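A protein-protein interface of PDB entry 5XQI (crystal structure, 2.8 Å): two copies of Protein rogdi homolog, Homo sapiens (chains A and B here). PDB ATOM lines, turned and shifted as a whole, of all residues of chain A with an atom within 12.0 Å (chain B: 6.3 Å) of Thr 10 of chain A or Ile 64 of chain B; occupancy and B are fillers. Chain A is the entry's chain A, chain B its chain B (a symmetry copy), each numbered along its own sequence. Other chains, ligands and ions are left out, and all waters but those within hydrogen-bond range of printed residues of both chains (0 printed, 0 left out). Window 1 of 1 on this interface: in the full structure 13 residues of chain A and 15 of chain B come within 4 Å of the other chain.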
ATOM      1  N   MET A   3     -24.264 -20.561   9.070  1.00  0.00           N
ATOM      2  CA  MET A   3     -24.019 -21.580  10.089  1.00  0.00           C
ATOM      3  C   MET A   3     -22.528 -21.825  10.290  1.00  0.00           C
ATOM      4  O   MET A   3     -22.075 -22.050  11.412  1.00  0.00           O
ATOM      5  CB  MET A   3     -24.713 -22.900   9.729  1.00  0.00           C
ATOM      6  CG  MET A   3     -24.328 -24.070  10.644  1.00  0.00           C
ATOM      7  SD  MET A   3     -24.708 -25.725  10.027  1.00  0.00           S
ATOM      8  CE  MET A   3     -26.498 -25.705  10.011  1.00  0.00           C
ATOM      9  N   ALA A   4     -21.767 -21.785   9.201  1.00  0.00           N
ATOM     10  CA  ALA A   4     -20.336 -22.040   9.279  1.00  0.00           C
ATOM     11  C   ALA A   4     -19.630 -20.801   9.808  1.00  0.00           C
ATOM     12  O   ALA A   4     -18.641 -20.898  10.537  1.00  0.00           O
ATOM     13  CB  ALA A   4     -19.792 -22.427   7.917  1.00  0.00           C
ATOM     14  N   THR A   5     -20.171 -19.637   9.457  1.00  0.00           N
ATOM     15  CA  THR A   5     -19.670 -18.364   9.956  1.00  0.00           C
ATOM     16  C   THR A   5     -19.875 -18.264  11.463  1.00  0.00           C
ATOM     17  O   THR A   5     -18.985 -17.825  12.192  1.00  0.00           O
ATOM     18  CB  THR A   5     -20.362 -17.173   9.266  1.00  0.00           C
ATOM     19  OG1 THR A   5     -21.773 -17.224   9.517  1.00  0.00           O
ATOM     20  CG2 THR A   5     -20.117 -17.213   7.770  1.00  0.00           C
ATOM     21  N   VAL A   6     -21.057 -18.670  11.921  1.00  0.00           N
ATOM     22  CA  VAL A   6     -21.359 -18.706  13.348  1.00  0.00           C
ATOM     23  C   VAL A   6     -20.382 -19.593  14.115  1.00  0.00           C
ATOM     24  O   VAL A   6     -19.798 -19.160  15.105  1.00  0.00           O
ATOM     25  CB  VAL A   6     -22.803 -19.185  13.614  1.00  0.00           C
ATOM     26  CG1 VAL A   6     -23.095 -19.215  15.110  1.00  0.00           C
ATOM     27  CG2 VAL A   6     -23.801 -18.298  12.880  1.00  0.00           C
ATOM     28  N   MET A   7     -20.206 -20.832  13.665  1.00  0.00           N
ATOM     29  CA  MET A   7     -19.300 -21.760  14.336  1.00  0.00           C
ATOM     30  C   MET A   7     -17.857 -21.262  14.310  1.00  0.00           C
ATOM     31  O   MET A   7     -17.092 -21.479  15.252  1.00  0.00           O
ATOM     32  CB  MET A   7     -19.375 -23.146  13.694  1.00  0.00           C
ATOM     33  CG  MET A   7     -18.777 -24.250  14.551  1.00  0.00           C
ATOM     34  SD  MET A   7     -19.421 -25.885  14.144  1.00  0.00           S
ATOM     35  CE  MET A   7     -21.145 -25.510  13.841  1.00  0.00           C
ATOM     36  N   ALA A   8     -17.494 -20.598  13.219  1.00  0.00           N
ATOM     37  CA  ALA A   8     -16.140 -20.085  13.034  1.00  0.00           C
ATOM     38  C   ALA A   8     -15.825 -18.874  13.913  1.00  0.00           C
ATOM     39  O   ALA A   8     -14.701 -18.731  14.395  1.00  0.00           O
ATOM     40  CB  ALA A   8     -15.910 -19.737  11.570  1.00  0.00           C
ATOM     41  N   ALA A   9     -16.820 -18.010  14.108  1.00  0.00           N
ATOM     42  CA  ALA A   9     -16.638 -16.745  14.824  1.00  0.00           C
ATOM     43  C   ALA A   9     -16.050 -16.909  16.222  1.00  0.00           C
ATOM     44  O   ALA A   9     -16.647 -17.534  17.092  1.00  0.00           O
ATOM     45  CB  ALA A   9     -17.967 -16.009  14.909  1.00  0.00           C
ATOM     46  N   THR A  10     -14.852 -16.359  16.410  1.00  0.00           N
ATOM     47  CA  THR A  10     -14.197 -16.321  17.715  1.00  0.00           C
ATOM     48  C   THR A  10     -14.454 -15.009  18.454  1.00  0.00           C
ATOM     49  O   THR A  10     -14.110 -13.934  17.963  1.00  0.00           O
ATOM     50  CB  THR A  10     -12.680 -16.525  17.582  1.00  0.00           C
ATOM     51  OG1 THR A  10     -12.420 -17.761  16.905  1.00  0.00           O
ATOM     52  CG2 THR A  10     -12.030 -16.568  18.955  1.00  0.00           C
ATOM     53  N   ALA A  11     -15.055 -15.105  19.638  1.00  0.00           N
ATOM     54  CA  ALA A  11     -15.349 -13.931  20.453  1.00  0.00           C
ATOM     55  C   ALA A  11     -14.079 -13.239  20.942  1.00  0.00           C
ATOM     56  O   ALA A  11     -13.024 -13.861  21.058  1.00  0.00           O
ATOM     57  CB  ALA A  11     -16.224 -14.321  21.639  1.00  0.00           C
ATOM     58  N   ALA A  12     -14.183 -11.941  21.208  1.00  0.00           N
ATOM     59  CA  ALA A  12     -13.077 -11.181  21.776  1.00  0.00           C
ATOM     60  C   ALA A  12     -12.804 -11.639  23.205  1.00  0.00           C
ATOM     61  O   ALA A  12     -13.732 -11.780  24.003  1.00  0.00           O
ATOM     62  CB  ALA A  12     -13.380  -9.688  21.738  1.00  0.00           C
ATOM     63  N   GLU A  13     -11.536 -11.872  23.530  1.00  0.00           N
ATOM     64  CA  GLU A  13     -11.191 -12.360  24.859  1.00  0.00           C
ATOM     65  C   GLU A  13     -11.286 -11.213  25.858  1.00  0.00           C
ATOM     66  O   GLU A  13     -11.015 -10.060  25.521  1.00  0.00           O
ATOM     67  CB  GLU A  13      -9.797 -12.984  24.877  1.00  0.00           C
ATOM     68  CG  GLU A  13      -9.648 -14.083  25.921  1.00  0.00           C
ATOM     69  CD  GLU A  13     -10.007 -15.454  25.384  1.00  0.00           C
ATOM     70  OE1 GLU A  13      -9.427 -15.868  24.358  1.00  0.00           O
ATOM     71  OE2 GLU A  13     -10.882 -16.115  25.984  1.00  0.00           O
ATOM     72  N   ARG A  14     -11.672 -11.539  27.088  1.00  0.00           N
ATOM     73  CA  ARG A  14     -11.856 -10.536  28.134  1.00  0.00           C
ATOM     74  C   ARG A  14     -10.537  -9.905  28.571  1.00  0.00           C
ATOM     75  O   ARG A  14      -9.500 -10.568  28.635  1.00  0.00           O
ATOM     76  CB  ARG A  14     -12.592 -11.160  29.327  1.00  0.00           C
ATOM     77  CG  ARG A  14     -13.071 -10.163  30.377  1.00  0.00           C
ATOM     78  CD  ARG A  14     -13.501 -10.830  31.690  1.00  0.00           C
ATOM     79  NE  ARG A  14     -12.415 -11.390  32.490  1.00  0.00           N
ATOM     80  CZ  ARG A  14     -12.227 -12.693  32.680  1.00  0.00           C
ATOM     81  NH1 ARG A  14     -13.054 -13.572  32.126  1.00  0.00           N
ATOM     82  NH2 ARG A  14     -11.218 -13.120  33.429  1.00  0.00           N
ATOM     83  N   GLN B  60     -18.646  -1.010  16.219  1.00  0.00           N
ATOM     84  CA  GLN B  60     -18.909  -2.433  16.019  1.00  0.00           C
ATOM     85  C   GLN B  60     -20.393  -2.704  15.792  1.00  0.00           C
ATOM     86  O   GLN B  60     -21.249  -2.087  16.428  1.00  0.00           O
ATOM     87  CB  GLN B  60     -18.413  -3.238  17.221  1.00  0.00           C
ATOM     88  CG  GLN B  60     -18.506  -4.745  17.052  1.00  0.00           C
ATOM     89  CD  GLN B  60     -17.829  -5.500  18.181  1.00  0.00           C
ATOM     90  OE1 GLN B  60     -17.054  -4.929  18.948  1.00  0.00           O
ATOM     91  NE2 GLN B  60     -18.121  -6.790  18.288  1.00  0.00           N
ATOM     92  N   ASN B  62     -21.355  -6.253  14.559  1.00  0.00           N
ATOM     93  CA  ASN B  62     -21.497  -7.694  14.719  1.00  0.00           C
ATOM     94  C   ASN B  62     -20.942  -8.171  16.051  1.00  0.00           C
ATOM     95  O   ASN B  62     -19.831  -7.812  16.437  1.00  0.00           O
ATOM     96  CB  ASN B  62     -20.810  -8.426  13.565  1.00  0.00           C
ATOM     97  CG  ASN B  62     -21.437  -8.107  12.222  1.00  0.00           C
ATOM     98  OD1 ASN B  62     -22.657  -7.988  12.109  1.00  0.00           O
ATOM     99  ND2 ASN B  62     -20.604  -7.961  11.198  1.00  0.00           N
ATOM    100  N   PHE B  63     -21.720  -8.987  16.750  1.00  0.00           N
ATOM    101  CA  PHE B  63     -21.347  -9.420  18.088  1.00  0.00           C
ATOM    102  C   PHE B  63     -21.474 -10.925  18.230  1.00  0.00           C
ATOM    103  O   PHE B  63     -22.447 -11.528  17.768  1.00  0.00           O
ATOM    104  CB  PHE B  63     -22.201  -8.703  19.136  1.00  0.00           C
ATOM    105  CG  PHE B  63     -22.051  -7.211  19.107  1.00  0.00           C
ATOM    106  CD1 PHE B  63     -20.995  -6.597  19.761  1.00  0.00           C
ATOM    107  CD2 PHE B  63     -22.947  -6.424  18.405  1.00  0.00           C
ATOM    108  CE1 PHE B  63     -20.844  -5.223  19.727  1.00  0.00           C
ATOM    109  CE2 PHE B  63     -22.802  -5.050  18.366  1.00  0.00           C
ATOM    110  CZ  PHE B  63     -21.749  -4.450  19.027  1.00  0.00           C
ATOM    111  N   ILE B  64     -20.489 -11.524  18.885  1.00  0.00           N
ATOM    112  CA  ILE B  64     -20.460 -12.963  19.064  1.00  0.00           C
ATOM    113  C   ILE B  64     -20.860 -13.333  20.488  1.00  0.00           C
ATOM    114  O   ILE B  64     -20.245 -12.897  21.462  1.00  0.00           O
ATOM    115  CB  ILE B  64     -19.060 -13.525  18.745  1.00  0.00           C
ATOM    116  CG1 ILE B  64     -18.622 -13.065  17.354  1.00  0.00           C
ATOM    117  CG2 ILE B  64     -19.040 -15.045  18.862  1.00  0.00           C
ATOM    118  CD1 ILE B  64     -17.143 -13.180  17.112  1.00  0.00           C
ATOM    119  N   LEU B  65     -21.908 -14.136  20.590  1.00  0.00           N
ATOM    120  CA  LEU B  65     -22.455 -14.562  21.864  1.00  0.00           C
ATOM    121  C   LEU B  65     -22.283 -16.069  22.015  1.00  0.00           C
ATOM    122  O   LEU B  65     -22.819 -16.842  21.217  1.00  0.00           O
ATOM    123  CB  LEU B  65     -23.936 -14.174  21.971  1.00  0.00           C
ATOM    124  CG  LEU B  65     -24.337 -12.701  22.158  1.00  0.00           C
ATOM    125  CD1 LEU B  65     -24.024 -11.835  20.939  1.00  0.00           C
ATOM    126  CD2 LEU B  65     -25.813 -12.590  22.520  1.00  0.00           C
ATOM    127  N   GLY B  66     -21.538 -16.487  23.033  1.00  0.00           N
ATOM    128  CA  GLY B  66     -21.358 -17.903  23.310  1.00  0.00           C
ATOM    129  C   GLY B  66     -20.085 -18.496  22.739  1.00  0.00           C
ATOM    130  O   GLY B  66     -19.479 -17.930  21.828  1.00  0.00           O
ATOM    131  N   LYS B  74     -24.793 -20.665  20.228  1.00  0.00           N
ATOM    132  CA  LYS B  74     -23.869 -19.647  19.768  1.00  0.00           C
ATOM    133  C   LYS B  74     -24.597 -18.755  18.783  1.00  0.00           C
ATOM    134  O   LYS B  74     -25.521 -19.194  18.103  1.00  0.00           O
ATOM    135  CB  LYS B  74     -22.629 -20.272  19.128  1.00  0.00           C
ATOM    136  CG  LYS B  74     -21.551 -19.255  18.801  1.00  0.00           C
ATOM    137  CD  LYS B  74     -20.248 -19.914  18.416  1.00  0.00           C
ATOM    138  CE  LYS B  74     -19.181 -18.868  18.189  1.00  0.00           C
ATOM    139  NZ  LYS B  74     -17.823 -19.461  18.081  1.00  0.00           N
ATOM    140  N   GLY B  75     -24.194 -17.495  18.717  1.00  0.00           N
ATOM    141  CA  GLY B  75     -24.940 -16.536  17.931  1.00  0.00           C
ATOM    142  C   GLY B  75     -24.086 -15.389  17.453  1.00  0.00           C
ATOM    143  O   GLY B  75     -23.177 -14.947  18.146  1.00  0.00           O
ATOM    144  N   VAL B  76     -24.364 -14.915  16.250  1.00  0.00           N
ATOM    145  CA  VAL B  76     -23.737 -13.702  15.769  1.00  0.00           C
ATOM    146  C   VAL B  76     -24.872 -12.747  15.490  1.00  0.00           C
ATOM    147  O   VAL B  76     -25.648 -12.934  14.550  1.00  0.00           O
ATOM    148  CB  VAL B  76     -22.871 -13.920  14.522  1.00  0.00           C
ATOM    149  CG1 VAL B  76     -22.284 -12.594  14.060  1.00  0.00           C
ATOM    150  CG2 VAL B  76     -21.755 -14.914  14.822  1.00  0.00           C
ATOM    151  N   LEU B  77     -24.988 -11.743  16.351  1.00  0.00           N
ATOM    152  CA  LEU B  77     -26.097 -10.809  16.279  1.00  0.00           C
ATOM    153  C   LEU B  77     -25.595  -9.463  15.794  1.00  0.00           C
ATOM    154  O   LEU B  77     -24.588  -8.942  16.279  1.00  0.00           O
ATOM    155  CB  LEU B  77     -26.799 -10.685  17.634  1.00  0.00           C
ATOM    156  CG  LEU B  77     -27.756 -11.821  18.025  1.00  0.00           C
ATOM    157  CD1 LEU B  77     -27.031 -13.137  18.297  1.00  0.00           C
ATOM    158  CD2 LEU B  77     -28.609 -11.417  19.219  1.00  0.00           C
ATOM    159  N   GLU B 250     -24.195 -14.107  26.267  1.00  0.00           N
ATOM    160  CA  GLU B 250     -24.149 -12.655  26.347  1.00  0.00           C
ATOM    161  C   GLU B 250     -22.854 -12.072  25.798  1.00  0.00           C
ATOM    162  O   GLU B 250     -21.845 -12.765  25.680  1.00  0.00           O
ATOM    163  CB  GLU B 250     -24.340 -12.216  27.798  1.00  0.00           C
ATOM    164  CG  GLU B 250     -23.293 -12.782  28.744  1.00  0.00           C
ATOM    165  CD  GLU B 250     -23.596 -12.487  30.198  1.00  0.00           C
ATOM    166  OE1 GLU B 250     -24.609 -11.807  30.470  1.00  0.00           O
ATOM    167  OE2 GLU B 250     -22.821 -12.937  31.068  1.00  0.00           O
ATOM    168  N   CYS B 251     -22.892 -10.789  25.463  1.00  0.00           N
ATOM    169  CA  CYS B 251     -21.720 -10.112  24.922  1.00  0.00           C
ATOM    170  C   CYS B 251     -21.731  -8.638  25.291  1.00  0.00           C
ATOM    171  O   CYS B 251     -22.765  -7.983  25.200  1.00  0.00           O
ATOM    172  CB  CYS B 251     -21.665 -10.274  23.400  1.00  0.00           C
ATOM    173  SG  CYS B 251     -20.426  -9.247  22.576  1.00  0.00           S
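O of Ala 9 of chain A lies within hydrogen-bond range of NZ of Lys 74 of chain B.
No residue of chain A comes within 4 Å of Phe 63 of chain B. Leu 65 of chain B touches none of the printed residues of chain A. No residue of chain A comes within 4 Å of Gly 66 of chain B. No residue of chain A comes within 4 Å of Gly 75 of chain B. Of chain A, only Ala 9 comes within 4 Å of Val 76 of chain B. Printed residues of chain B within 4 Å of Ala 11 of chain A: Ile 64 (3.8 Å). Of the printed residues of chain B, Met 7 of chain A touches Lys 74 (3.6 Å). Leu 77 of chain B touches none of the printed residues of chain A. The nearest residue of chain A that does not touch Ile 64 of chain B is Ala 12 of chain A (5.2 Å). The nearest printed residue of chain B that does not touch Val 6 of chain A is Val 76 of chain B (4.1 Å).
No position is printed for both chains.
Among the printed residues, pairs that only touch across the chains: Val 6 of chain A with Lys 74 of chain B, Met 7 of chain A with Lys 74 of chain B, Ala 9 of chain A with Ile 64 of chain B, Ala 9 of chain A with Val 76 of chain B, Thr 10 of chain A with Ile 64 of chain B and Ala 11 of chain A with Ile 64 of chain B.
Of the 12 printed residues of chain A, 5 touch a printed residue of chain B. Printed residues of chain A that touch a printed residue of chain B: Val 6, Met 7, Ala 9, Thr 10 and Ala 11. Hydrophobic or aromatic side chains of chain A within 4 Å of the printed part of chain B: Val 6 and Ala 9. Among the printed residues, no Asp or Glu carboxylate lies within 4 Å of a Lys or Arg side-chain nitrogen of the other chain.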
